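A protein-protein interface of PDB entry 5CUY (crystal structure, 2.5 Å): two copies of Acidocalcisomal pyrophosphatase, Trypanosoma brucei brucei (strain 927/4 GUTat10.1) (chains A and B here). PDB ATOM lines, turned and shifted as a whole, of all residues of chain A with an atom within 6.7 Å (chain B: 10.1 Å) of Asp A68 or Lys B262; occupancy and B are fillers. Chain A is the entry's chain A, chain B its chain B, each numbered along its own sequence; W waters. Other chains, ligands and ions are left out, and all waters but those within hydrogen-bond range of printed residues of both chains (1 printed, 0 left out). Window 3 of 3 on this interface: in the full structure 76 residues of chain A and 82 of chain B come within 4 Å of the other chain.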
ATOM      1  N   ARG A  57      10.008 -18.111   3.387  1.00  0.00           N
ATOM      2  CA  ARG A  57       9.935 -18.826   4.673  1.00  0.00           C
ATOM      3  C   ARG A  57      10.403 -20.259   4.610  1.00  0.00           C
ATOM      4  O   ARG A  57      10.900 -20.790   5.587  1.00  0.00           O
ATOM      5  CB  ARG A  57       8.497 -18.825   5.211  1.00  0.00           C
ATOM      6  CG  ARG A  57       7.999 -17.466   5.672  1.00  0.00           C
ATOM      7  CD  ARG A  57       8.684 -17.076   6.944  1.00  0.00           C
ATOM      8  NE  ARG A  57       7.744 -17.048   8.054  1.00  0.00           N
ATOM      9  CZ  ARG A  57       7.617 -18.003   8.970  1.00  0.00           C
ATOM     10  NH1 ARG A  57       6.723 -17.865   9.935  1.00  0.00           N
ATOM     11  NH2 ARG A  57       8.381 -19.089   8.934  1.00  0.00           N
ATOM     12  N   VAL A  59       8.276 -22.626   3.862  1.00  0.00           N
ATOM     13  CA  VAL A  59       7.109 -23.164   4.549  1.00  0.00           C
ATOM     14  C   VAL A  59       5.960 -23.247   3.521  1.00  0.00           C
ATOM     15  O   VAL A  59       5.730 -22.314   2.754  1.00  0.00           O
ATOM     16  CB  VAL A  59       6.729 -22.199   5.717  1.00  0.00           C
ATOM     17  CG1 VAL A  59       5.498 -22.699   6.455  1.00  0.00           C
ATOM     18  CG2 VAL A  59       7.948 -22.018   6.666  1.00  0.00           C
ATOM     19  N   ASP A  63       0.688 -24.327   5.427  1.00  0.00           N
ATOM     20  CA  ASP A  63       1.253 -24.430   6.776  1.00  0.00           C
ATOM     21  C   ASP A  63       1.264 -23.015   7.325  1.00  0.00           C
ATOM     22  O   ASP A  63       0.986 -22.740   8.503  1.00  0.00           O
ATOM     23  CB  ASP A  63       2.690 -24.974   6.700  1.00  0.00           C
ATOM     24  CG  ASP A  63       2.776 -26.492   6.914  1.00  0.00           C
ATOM     25  OD1 ASP A  63       1.743 -27.123   7.125  1.00  0.00           O
ATOM     26  OD2 ASP A  63       3.887 -27.077   6.888  1.00  0.00           O
ATOM     27  N   LEU A  64       1.603 -22.098   6.440  1.00  0.00           N
ATOM     28  CA  LEU A  64       1.649 -20.699   6.801  1.00  0.00           C
ATOM     29  C   LEU A  64       0.273 -20.166   7.236  1.00  0.00           C
ATOM     30  O   LEU A  64       0.153 -19.485   8.254  1.00  0.00           O
ATOM     31  CB  LEU A  64       2.171 -19.903   5.603  1.00  0.00           C
ATOM     32  CG  LEU A  64       3.212 -18.855   5.944  1.00  0.00           C
ATOM     33  CD1 LEU A  64       4.431 -19.523   6.576  1.00  0.00           C
ATOM     34  CD2 LEU A  64       3.557 -18.131   4.673  1.00  0.00           C
ATOM     35  N   ALA A  65      -0.760 -20.453   6.461  1.00  0.00           N
ATOM     36  CA  ALA A  65      -2.084 -19.974   6.807  1.00  0.00           C
ATOM     37  C   ALA A  65      -2.616 -20.631   8.085  1.00  0.00           C
ATOM     38  O   ALA A  65      -3.382 -20.056   8.838  1.00  0.00           O
ATOM     39  CB  ALA A  65      -3.051 -20.211   5.629  1.00  0.00           C
ATOM     40  N   ALA A  66      -2.200 -21.854   8.325  1.00  0.00           N
ATOM     41  CA  ALA A  66      -2.652 -22.593   9.483  1.00  0.00           C
ATOM     42  C   ALA A  66      -1.870 -22.260  10.754  1.00  0.00           C
ATOM     43  O   ALA A  66      -2.451 -22.067  11.821  1.00  0.00           O
ATOM     44  CB  ALA A  66      -2.513 -24.078   9.199  1.00  0.00           C
ATOM     45  N   TYR A  67      -0.555 -22.151  10.627  1.00  0.00           N
ATOM     46  CA  TYR A  67       0.249 -21.992  11.798  1.00  0.00           C
ATOM     47  C   TYR A  67       1.062 -20.790  12.045  1.00  0.00           C
ATOM     48  O   TYR A  67       1.576 -20.642  13.133  1.00  0.00           O
ATOM     49  CB  TYR A  67       1.169 -23.181  11.922  1.00  0.00           C
ATOM     50  CG  TYR A  67       0.467 -24.479  11.788  1.00  0.00           C
ATOM     51  CD1 TYR A  67      -0.436 -24.912  12.753  1.00  0.00           C
ATOM     52  CD2 TYR A  67       0.728 -25.303  10.695  1.00  0.00           C
ATOM     53  CE1 TYR A  67      -1.054 -26.144  12.624  1.00  0.00           C
ATOM     54  CE2 TYR A  67       0.123 -26.527  10.556  1.00  0.00           C
ATOM     55  CZ  TYR A  67      -0.759 -26.953  11.507  1.00  0.00           C
ATOM     56  OH  TYR A  67      -1.333 -28.183  11.328  1.00  0.00           O
ATOM     57  N   ASP A  68       1.232 -19.950  11.055  1.00  0.00           N
ATOM     58  CA  ASP A  68       2.009 -18.775  11.304  1.00  0.00           C
ATOM     59  C   ASP A  68       1.209 -17.824  12.190  1.00  0.00           C
ATOM     60  O   ASP A  68      -0.024 -17.759  12.143  1.00  0.00           O
ATOM     61  CB  ASP A  68       2.353 -18.063  10.010  1.00  0.00           C
ATOM     62  CG  ASP A  68       3.268 -16.876  10.251  1.00  0.00           C
ATOM     63  OD1 ASP A  68       4.454 -17.141  10.584  1.00  0.00           O
ATOM     64  OD2 ASP A  68       2.819 -15.698  10.146  1.00  0.00           O
ATOM     65  N   LYS A  69       1.916 -17.084  13.011  1.00  0.00           N
ATOM     66  CA  LYS A  69       1.229 -16.132  13.847  1.00  0.00           C
ATOM     67  C   LYS A  69       0.394 -15.106  13.033  1.00  0.00           C
ATOM     68  O   LYS A  69      -0.773 -14.867  13.337  1.00  0.00           O
ATOM     69  CB  LYS A  69       2.244 -15.414  14.770  1.00  0.00           C
ATOM     70  CG  LYS A  69       3.625 -15.138  14.181  1.00  0.00           C
ATOM     71  CD  LYS A  69       4.375 -14.069  14.996  1.00  0.00           C
ATOM     72  CE  LYS A  69       3.920 -12.642  14.595  1.00  0.00           C
ATOM     73  NZ  LYS A  69       4.711 -11.970  13.479  1.00  0.00           N
ATOM     74  N   ASP A  70       0.947 -14.507  11.990  1.00  0.00           N
ATOM     75  CA  ASP A  70       0.142 -13.531  11.263  1.00  0.00           C
ATOM     76  C   ASP A  70      -0.862 -14.033  10.188  1.00  0.00           C
ATOM     77  O   ASP A  70      -0.742 -15.132   9.638  1.00  0.00           O
ATOM     78  CB  ASP A  70       1.068 -12.481  10.650  1.00  0.00           C
ATOM     79  CG  ASP A  70       1.831 -11.684  11.707  1.00  0.00           C
ATOM     80  OD1 ASP A  70       1.226 -11.228  12.718  1.00  0.00           O
ATOM     81  OD2 ASP A  70       3.049 -11.507  11.499  1.00  0.00           O
ATOM     82  N   ASP A  71      -1.867 -13.216   9.903  1.00  0.00           N
ATOM     83  CA  ASP A  71      -2.842 -13.544   8.873  1.00  0.00           C
ATOM     84  C   ASP A  71      -2.150 -13.218   7.562  1.00  0.00           C
ATOM     85  O   ASP A  71      -1.144 -12.480   7.559  1.00  0.00           O
ATOM     86  CB  ASP A  71      -4.059 -12.639   8.982  1.00  0.00           C
ATOM     87  CG  ASP A  71      -5.146 -13.198   9.900  1.00  0.00           C
ATOM     88  OD1 ASP A  71      -5.003 -14.324  10.445  1.00  0.00           O
ATOM     89  OD2 ASP A  71      -6.172 -12.484  10.058  1.00  0.00           O
ATOM     90  N   PHE A  72      -2.649 -13.784   6.460  1.00  0.00           N
ATOM     91  CA  PHE A  72      -2.112 -13.456   5.133  1.00  0.00           C
ATOM     92  C   PHE A  72      -2.387 -11.973   4.887  1.00  0.00           C
ATOM     93  O   PHE A  72      -3.444 -11.496   5.260  1.00  0.00           O
ATOM     94  CB  PHE A  72      -2.861 -14.203   4.041  1.00  0.00           C
ATOM     95  CG  PHE A  72      -2.236 -15.480   3.644  1.00  0.00           C
ATOM     96  CD1 PHE A  72      -1.678 -16.321   4.600  1.00  0.00           C
ATOM     97  CD2 PHE A  72      -2.271 -15.884   2.323  1.00  0.00           C
ATOM     98  CE1 PHE A  72      -1.167 -17.548   4.266  1.00  0.00           C
ATOM     99  CE2 PHE A  72      -1.755 -17.130   1.968  1.00  0.00           C
ATOM    100  CZ  PHE A  72      -1.205 -17.958   2.944  1.00  0.00           C
ATOM    101  N   ILE B 230     -15.441 -29.053  14.646  1.00  0.00           N
ATOM    102  CA  ILE B 230     -13.995 -28.959  14.738  1.00  0.00           C
ATOM    103  C   ILE B 230     -13.575 -30.142  15.553  1.00  0.00           C
ATOM    104  O   ILE B 230     -13.853 -30.185  16.743  1.00  0.00           O
ATOM    105  CB  ILE B 230     -13.632 -27.678  15.442  1.00  0.00           C
ATOM    106  CG1 ILE B 230     -14.151 -26.532  14.589  1.00  0.00           C
ATOM    107  CG2 ILE B 230     -12.145 -27.584  15.688  1.00  0.00           C
ATOM    108  CD1 ILE B 230     -13.668 -25.171  14.978  1.00  0.00           C
ATOM    109  N   THR B 234      -7.592 -30.450  16.602  1.00  0.00           N
ATOM    110  CA  THR B 234      -7.416 -29.762  15.333  1.00  0.00           C
ATOM    111  C   THR B 234      -7.766 -28.306  15.440  1.00  0.00           C
ATOM    112  O   THR B 234      -8.357 -27.889  16.432  1.00  0.00           O
ATOM    113  CB  THR B 234      -8.247 -30.427  14.233  1.00  0.00           C
ATOM    114  OG1 THR B 234      -9.646 -30.292  14.526  1.00  0.00           O
ATOM    115  CG2 THR B 234      -7.885 -31.897  14.158  1.00  0.00           C
ATOM    116  N   ARG B 235      -7.394 -27.502  14.450  1.00  0.00           N
ATOM    117  CA  ARG B 235      -7.717 -26.099  14.561  1.00  0.00           C
ATOM    118  C   ARG B 235      -8.310 -25.494  13.329  1.00  0.00           C
ATOM    119  O   ARG B 235      -8.562 -24.286  13.312  1.00  0.00           O
ATOM    120  CB  ARG B 235      -6.502 -25.286  14.997  1.00  0.00           C
ATOM    121  CG  ARG B 235      -5.399 -25.189  13.959  1.00  0.00           C
ATOM    122  CD  ARG B 235      -4.152 -24.446  14.486  1.00  0.00           C
ATOM    123  NE  ARG B 235      -3.491 -25.136  15.600  1.00  0.00           N
ATOM    124  CZ  ARG B 235      -2.500 -24.632  16.345  1.00  0.00           C
ATOM    125  NH1 ARG B 235      -2.037 -23.422  16.114  1.00  0.00           N
ATOM    126  NH2 ARG B 235      -1.971 -25.347  17.323  1.00  0.00           N
ATOM    127  N   ALA B 236      -8.520 -26.284  12.290  1.00  0.00           N
ATOM    128  CA  ALA B 236      -9.150 -25.723  11.096  1.00  0.00           C
ATOM    129  C   ALA B 236     -10.636 -25.534  11.384  1.00  0.00           C
ATOM    130  O   ALA B 236     -11.259 -26.413  11.954  1.00  0.00           O
ATOM    131  CB  ALA B 236      -8.993 -26.646   9.946  1.00  0.00           C
ATOM    132  N   LYS B 237     -11.209 -24.413  10.974  1.00  0.00           N
ATOM    133  CA  LYS B 237     -12.621 -24.139  11.238  1.00  0.00           C
ATOM    134  C   LYS B 237     -13.654 -24.611  10.205  1.00  0.00           C
ATOM    135  O   LYS B 237     -13.492 -24.419   9.003  1.00  0.00           O
ATOM    136  CB  LYS B 237     -12.838 -22.646  11.438  1.00  0.00           C
ATOM    137  CG  LYS B 237     -12.106 -22.044  12.621  1.00  0.00           C
ATOM    138  CD  LYS B 237     -12.406 -20.560  12.655  1.00  0.00           C
ATOM    139  CE  LYS B 237     -11.976 -19.908  13.952  1.00  0.00           C
ATOM    140  NZ  LYS B 237     -12.337 -18.464  13.936  1.00  0.00           N
ATOM    141  N   VAL B 257      -8.772 -18.318   1.348  1.00  0.00           N
ATOM    142  CA  VAL B 257      -7.802 -18.898   2.257  1.00  0.00           C
ATOM    143  C   VAL B 257      -8.499 -19.542   3.438  1.00  0.00           C
ATOM    144  O   VAL B 257      -9.329 -18.933   4.077  1.00  0.00           O
ATOM    145  CB  VAL B 257      -6.879 -17.846   2.798  1.00  0.00           C
ATOM    146  CG1 VAL B 257      -5.764 -18.517   3.555  1.00  0.00           C
ATOM    147  CG2 VAL B 257      -6.362 -16.972   1.670  1.00  0.00           C
ATOM    148  N   PRO B 258      -8.214 -20.793   3.725  1.00  0.00           N
ATOM    149  CA  PRO B 258      -8.918 -21.348   4.903  1.00  0.00           C
ATOM    150  C   PRO B 258      -8.529 -20.671   6.274  1.00  0.00           C
ATOM    151  O   PRO B 258      -7.381 -20.348   6.511  1.00  0.00           O
ATOM    152  CB  PRO B 258      -8.539 -22.831   4.861  1.00  0.00           C
ATOM    153  CG  PRO B 258      -7.231 -22.868   4.088  1.00  0.00           C
ATOM    154  CD  PRO B 258      -7.405 -21.808   3.028  1.00  0.00           C
ATOM    155  N   ARG B 259      -9.500 -20.483   7.159  1.00  0.00           N
ATOM    156  CA  ARG B 259      -9.294 -19.866   8.455  1.00  0.00           C
ATOM    157  C   ARG B 259      -8.964 -20.897   9.551  1.00  0.00           C
ATOM    158  O   ARG B 259      -9.366 -22.053   9.443  1.00  0.00           O
ATOM    159  CB  ARG B 259     -10.548 -19.107   8.866  1.00  0.00           C
ATOM    160  CG  ARG B 259     -10.908 -17.891   8.035  1.00  0.00           C
ATOM    161  CD  ARG B 259     -10.721 -16.634   8.855  1.00  0.00           C
ATOM    162  NE  ARG B 259     -11.860 -15.735   8.723  1.00  0.00           N
ATOM    163  CZ  ARG B 259     -12.977 -15.813   9.446  1.00  0.00           C
ATOM    164  NH1 ARG B 259     -13.114 -16.752  10.384  1.00  0.00           N
ATOM    165  NH2 ARG B 259     -13.982 -14.963   9.201  1.00  0.00           N
ATOM    166  N   PHE B 260      -8.258 -20.468  10.600  1.00  0.00           N
ATOM    167  CA  PHE B 260      -7.871 -21.363  11.673  1.00  0.00           C
ATOM    168  C   PHE B 260      -7.891 -20.675  13.044  1.00  0.00           C
ATOM    169  O   PHE B 260      -7.837 -19.448  13.117  1.00  0.00           O
ATOM    170  CB  PHE B 260      -6.456 -21.933  11.414  1.00  0.00           C
ATOM    171  CG  PHE B 260      -6.302 -22.719  10.088  1.00  0.00           C
ATOM    172  CD1 PHE B 260      -6.064 -22.049   8.869  1.00  0.00           C
ATOM    173  CD2 PHE B 260      -6.315 -24.123  10.086  1.00  0.00           C
ATOM    174  CE1 PHE B 260      -5.830 -22.760   7.684  1.00  0.00           C
ATOM    175  CE2 PHE B 260      -6.083 -24.859   8.911  1.00  0.00           C
ATOM    176  CZ  PHE B 260      -5.837 -24.177   7.708  1.00  0.00           C
ATOM    177  N   TYR B 261      -8.019 -21.432  14.137  1.00  0.00           N
ATOM    178  CA  TYR B 261      -7.972 -20.770  15.454  1.00  0.00           C
ATOM    179  C   TYR B 261      -6.481 -20.470  15.650  1.00  0.00           C
ATOM    180  O   TYR B 261      -5.675 -21.380  15.536  1.00  0.00           O
ATOM    181  CB  TYR B 261      -8.451 -21.709  16.578  1.00  0.00           C
ATOM    182  CG  TYR B 261      -9.960 -21.761  16.766  1.00  0.00           C
ATOM    183  CD1 TYR B 261     -10.676 -20.650  17.234  1.00  0.00           C
ATOM    184  CD2 TYR B 261     -10.686 -22.889  16.369  1.00  0.00           C
ATOM    185  CE1 TYR B 261     -12.067 -20.653  17.277  1.00  0.00           C
ATOM    186  CE2 TYR B 261     -12.084 -22.910  16.411  1.00  0.00           C
ATOM    187  CZ  TYR B 261     -12.770 -21.796  16.853  1.00  0.00           C
ATOM    188  OH  TYR B 261     -14.163 -21.827  16.825  1.00  0.00           O
ATOM    189  N   LYS B 262      -6.076 -19.234  15.902  1.00  0.00           N
ATOM    190  CA  LYS B 262      -4.645 -19.034  16.093  1.00  0.00           C
ATOM    191  C   LYS B 262      -4.077 -19.311  17.511  1.00  0.00           C
ATOM    192  O   LYS B 262      -2.893 -19.508  17.672  1.00  0.00           O
ATOM    193  CB  LYS B 262      -4.267 -17.643  15.635  1.00  0.00           C
ATOM    194  CG  LYS B 262      -4.447 -17.463  14.131  1.00  0.00           C
ATOM    195  CD  LYS B 262      -3.369 -18.210  13.359  1.00  0.00           C
ATOM    196  CE  LYS B 262      -3.712 -18.373  11.871  1.00  0.00           C
ATOM    197  NZ  LYS B 262      -2.433 -18.492  11.066  1.00  0.00           N
ATOM    198  N   HIS B 263      -4.925 -19.370  18.525  1.00  0.00           N
ATOM    199  CA  HIS B 263      -4.501 -19.611  19.911  1.00  0.00           C
ATOM    200  C   HIS B 263      -3.829 -20.963  20.138  1.00  0.00           C
ATOM    201  O   HIS B 263      -2.900 -21.086  20.959  1.00  0.00           O
ATOM    202  CB  HIS B 263      -5.716 -19.508  20.846  1.00  0.00           C
ATOM    203  CG  HIS B 263      -5.420 -19.870  22.267  1.00  0.00           C
ATOM    204  ND1 HIS B 263      -4.468 -19.213  23.025  1.00  0.00           N
ATOM    205  CD2 HIS B 263      -5.944 -20.829  23.069  1.00  0.00           C
ATOM    206  CE1 HIS B 263      -4.417 -19.758  24.229  1.00  0.00           C
ATOM    207  NE2 HIS B 263      -5.302 -20.741  24.282  1.00  0.00           N
ATOM    208  N   GLY B 264      -4.306 -21.972  19.411  1.00  0.00           N
ATOM    209  CA  GLY B 264      -3.779 -23.323  19.543  1.00  0.00           C
ATOM    210  C   GLY B 264      -4.901 -24.233  19.124  1.00  0.00           C
ATOM    211  O   GLY B 264      -5.922 -23.736  18.713  1.00  0.00           O
ATOM    212  N   ASP B 265      -4.770 -25.539  19.227  1.00  0.00           N
ATOM    213  CA  ASP B 265      -5.883 -26.379  18.782  1.00  0.00           C
ATOM    214  C   ASP B 265      -6.990 -26.491  19.818  1.00  0.00           C
ATOM    215  O   ASP B 265      -6.774 -26.293  21.014  1.00  0.00           O
ATOM    216  CB  ASP B 265      -5.388 -27.793  18.423  1.00  0.00           C
ATOM    217  CG  ASP B 265      -4.233 -27.781  17.384  1.00  0.00           C
ATOM    218  OD1 ASP B 265      -4.520 -27.478  16.194  1.00  0.00           O
ATOM    219  OD2 ASP B 265      -3.050 -28.069  17.751  1.00  0.00           O
ATOM    220  N   MET B 266      -8.193 -26.762  19.327  1.00  0.00           N
ATOM    221  CA  MET B 266      -9.343 -27.032  20.179  1.00  0.00           C
ATOM    222  C   MET B 266      -8.943 -28.413  20.766  1.00  0.00           C
ATOM    223  O   MET B 266      -8.529 -29.306  20.027  1.00  0.00           O
ATOM    224  CB  MET B 266     -10.592 -27.114  19.282  1.00  0.00           C
ATOM    225  CG  MET B 266     -11.915 -27.408  19.955  1.00  0.00           C
ATOM    226  SD  MET B 266     -12.348 -26.498  21.490  1.00  0.00           S
ATOM    227  CE  MET B 266     -12.406 -24.866  20.887  1.00  0.00           C
ATOM    228  N   TRP B 364      -9.101 -21.909  27.878  1.00  0.00           N
ATOM    229  CA  TRP B 364      -9.071 -21.769  26.435  1.00  0.00           C
ATOM    230  C   TRP B 364     -10.018 -20.677  26.001  1.00  0.00           C
ATOM    231  O   TRP B 364      -9.631 -19.799  25.237  1.00  0.00           O
ATOM    232  CB  TRP B 364      -9.465 -23.093  25.755  1.00  0.00           C
ATOM    233  CG  TRP B 364      -8.924 -23.237  24.377  1.00  0.00           C
ATOM    234  CD1 TRP B 364      -7.747 -23.862  24.013  1.00  0.00           C
ATOM    235  CD2 TRP B 364      -9.537 -22.782  23.146  1.00  0.00           C
ATOM    236  NE1 TRP B 364      -7.606 -23.825  22.628  1.00  0.00           N
ATOM    237  CE2 TRP B 364      -8.688 -23.174  22.080  1.00  0.00           C
ATOM    238  CE3 TRP B 364     -10.713 -22.098  22.842  1.00  0.00           C
ATOM    239  CZ2 TRP B 364      -9.001 -22.898  20.728  1.00  0.00           C
ATOM    240  CZ3 TRP B 364     -11.021 -21.826  21.477  1.00  0.00           C
ATOM    241  CH2 TRP B 364     -10.168 -22.230  20.457  1.00  0.00           C
ATOM    242  N   VAL B 367      -8.945 -16.999  26.917  1.00  0.00           N
ATOM    243  CA  VAL B 367      -7.863 -16.346  26.210  1.00  0.00           C
ATOM    244  C   VAL B 367      -7.654 -16.492  24.708  1.00  0.00           C
ATOM    245  O   VAL B 367      -6.775 -15.828  24.144  1.00  0.00           O
ATOM    246  CB  VAL B 367      -6.516 -16.697  26.912  1.00  0.00           C
ATOM    247  CG1 VAL B 367      -6.629 -16.425  28.490  1.00  0.00           C
ATOM    248  CG2 VAL B 367      -6.163 -18.154  26.640  1.00  0.00           C
ATOM    249  N   TYR B 368      -8.461 -17.304  24.042  1.00  0.00           N
ATOM    250  CA  TYR B 368      -8.227 -17.501  22.617  1.00  0.00           C
ATOM    251  C   TYR B 368      -8.166 -16.261  21.730  1.00  0.00           C
ATOM    252  O   TYR B 368      -7.718 -16.358  20.613  1.00  0.00           O
ATOM    253  CB  TYR B 368      -9.204 -18.527  22.022  1.00  0.00           C
ATOM    254  CG  TYR B 368     -10.593 -18.023  21.753  1.00  0.00           C
ATOM    255  CD1 TYR B 368     -11.449 -17.694  22.803  1.00  0.00           C
ATOM    256  CD2 TYR B 368     -11.070 -17.900  20.450  1.00  0.00           C
ATOM    257  CE1 TYR B 368     -12.736 -17.262  22.576  1.00  0.00           C
ATOM    258  CE2 TYR B 368     -12.374 -17.467  20.208  1.00  0.00           C
ATOM    259  CZ  TYR B 368     -13.195 -17.155  21.281  1.00  0.00           C
ATOM    260  OH  TYR B 368     -14.490 -16.781  21.075  1.00  0.00           O
ATOM    261  N   LYS B 369      -8.579 -15.097  22.210  1.00  0.00           N
ATOM    262  CA  LYS B 369      -8.498 -13.891  21.367  1.00  0.00           C
ATOM    263  C   LYS B 369      -7.289 -12.986  21.714  1.00  0.00           C
ATOM    264  O   LYS B 369      -7.054 -11.968  21.049  1.00  0.00           O
ATOM    265  CB  LYS B 369      -9.781 -13.058  21.480  1.00  0.00           C
ATOM    266  CG  LYS B 369     -11.020 -13.789  21.141  1.00  0.00           C
ATOM    267  CD  LYS B 369     -12.196 -12.842  21.088  1.00  0.00           C
ATOM    268  CE  LYS B 369     -12.768 -12.426  22.480  1.00  0.00           C
ATOM    269  NZ  LYS B 369     -14.051 -11.602  22.354  1.00  0.00           N
ATOM    270  N   ILE B 370      -6.534 -13.336  22.757  1.00  0.00           N
ATOM    271  CA  ILE B 370      -5.372 -12.533  23.115  1.00  0.00           C
ATOM    272  C   ILE B 370      -4.315 -12.649  21.997  1.00  0.00           C
ATOM    273  O   ILE B 370      -3.743 -11.634  21.563  1.00  0.00           O
ATOM    274  CB  ILE B 370      -4.803 -12.967  24.514  1.00  0.00           C
ATOM    275  CG1 ILE B 370      -5.768 -12.512  25.613  1.00  0.00           C
ATOM    276  CG2 ILE B 370      -3.455 -12.384  24.752  1.00  0.00           C
ATOM    277  CD1 ILE B 370      -5.413 -12.962  27.083  1.00  0.00           C
ATOM    278  N   CYS B 371      -4.071 -13.877  21.527  1.00  0.00           N
ATOM    279  CA  CYS B 371      -3.108 -14.156  20.457  1.00  0.00           C
ATOM    280  C   CYS B 371      -3.072 -13.039  19.385  1.00  0.00           C
ATOM    281  O   CYS B 371      -2.027 -12.452  19.098  1.00  0.00           O
ATOM    282  CB  CYS B 371      -3.443 -15.506  19.755  1.00  0.00           C
ATOM    283  SG  CYS B 371      -1.969 -16.208  18.774  1.00  0.00           S
ATOM    284  N   GLN B 372      -4.230 -12.761  18.803  1.00  0.00           N
ATOM    285  CA  GLN B 372      -4.324 -11.769  17.760  1.00  0.00           C
ATOM    286  C   GLN B 372      -4.611 -10.315  18.164  1.00  0.00           C
ATOM    287  O   GLN B 372      -5.111  -9.558  17.334  1.00  0.00           O
ATOM    288  CB  GLN B 372      -5.371 -12.197  16.755  1.00  0.00           C
ATOM    289  CG  GLN B 372      -5.084 -13.511  16.065  1.00  0.00           C
ATOM    290  CD  GLN B 372      -6.389 -14.216  15.702  1.00  0.00           C
ATOM    291  OE1 GLN B 372      -7.300 -14.382  16.562  1.00  0.00           O
ATOM    292  NE2 GLN B 372      -6.500 -14.632  14.438  1.00  0.00           N
ATOM    293  N   GLY B 373      -4.304  -9.929  19.413  1.00  0.00           N
ATOM    294  CA  GLY B 373      -4.497  -8.558  19.857  1.00  0.00           C
ATOM    295  C   GLY B 373      -5.792  -8.236  20.572  1.00  0.00           C
ATOM    296  O   GLY B 373      -6.099  -7.064  20.759  1.00  0.00           O
HETATM  297  O   HOH W   1       0.809 -22.183  15.414  1.00  0.00           O
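The backbone carbonyl oxygen of Ala A65 lies within hydrogen-bond range of the side-chain amino group of Lys B262 (2.9 Å).
The side-chain amino group (NZ) of Lys B262 is in hydrogen-bond range of the backbone carbonyl oxygen (O) of Asp A68.
OD1 of Asp A68 lies within salt-bridge range of NH1 of Arg A57, at 2.5 Å.
The side-chain carboxylate (OD2) of Asp A68 lies within hydrogen-bond range of the backbone NH (N) of Asp A70 (2.9 Å).
O of Arg B235 sits at hydrogen-bond distance from N of Tyr B261 (3.0 Å).
NE of Arg B235 lies within salt-bridge range of OD1 of Asp B265 (2.6 Å).
O of Lys B262 is in hydrogen-bond range of SG of Cys B371, at 3.6 Å.
Leu A64 touches Lys B262 (O to NZ, 3.9 Å).
Ala A65 touches Val B257 (CB to CG1, 3.8 Å).
Ala A65 touches Phe B260 (O to CD1, 3.3 Å).
Arg B235 touches Ala A66 (CD to O, 3.96 Å).
Ala A66 touches Phe B260.
Ala A66 touches Lys B262 (O to NZ, 3.7 Å).
Arg B235 touches Tyr A67 (NE to CE1, 3.98 Å).
Of chain B, only Val B257 (3.8 Å), Phe B260 (3.3 Å) and Lys B262 (2.9 Å) come within 4 Å of Ala A65.
Of the printed residues of chain B, Tyr A67 touches Arg B235.
Asp A68 touches one residue of chain B.
No residue of chain B comes within 4 Å of Lys A69.
No residue of chain B comes within 4 Å of Asp A70.
Of the printed residues of chain A, Arg B235 touches Ala A66 (3.96 Å) and Tyr A67 (3.98 Å).
Printed residues of chain A within 4 Å of Val B257: Ala A65.
Printed residues of chain A within 4 Å of Phe B260: Ala A65 and Ala A66.
Printed residues of chain A within 4 Å of Lys B262: Leu A64, Ala A65, Ala A66 and Asp A68.
The nearest residue of chain B that does not touch Asp A68 is Arg B235 (7.0 Å).
The nearest printed residue of chain A that does not touch Arg B235 is Asp A68 (7.0 Å).
Of the 23 printed residues of chain B, 4 touch a printed residue of chain A.
Printed residues of chain B that touch a printed residue of chain A: Arg B235, Val B257, Phe B260 and Lys B262.
Of the 12 printed residues of chain A, 5 touch a printed residue of chain B.
Hydrophobic or aromatic side chains of chain A that line the printed part of chain B: Ala A65, Ala A66 and Tyr A67.
Among the printed residues, no Asp or Glu carboxylate lies within 4 Å of a Lys or Arg side-chain nitrogen of the other chain.
No position is printed for both chains.
Of the 9 pairs that touch across the chains among the printed residues, none has its exchanged pair printed and touching as well.
Water W1 lies within hydrogen-bond range of O of Tyr A67 (2.9 Å) and NH1 of Arg B235 (3.2 Å).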
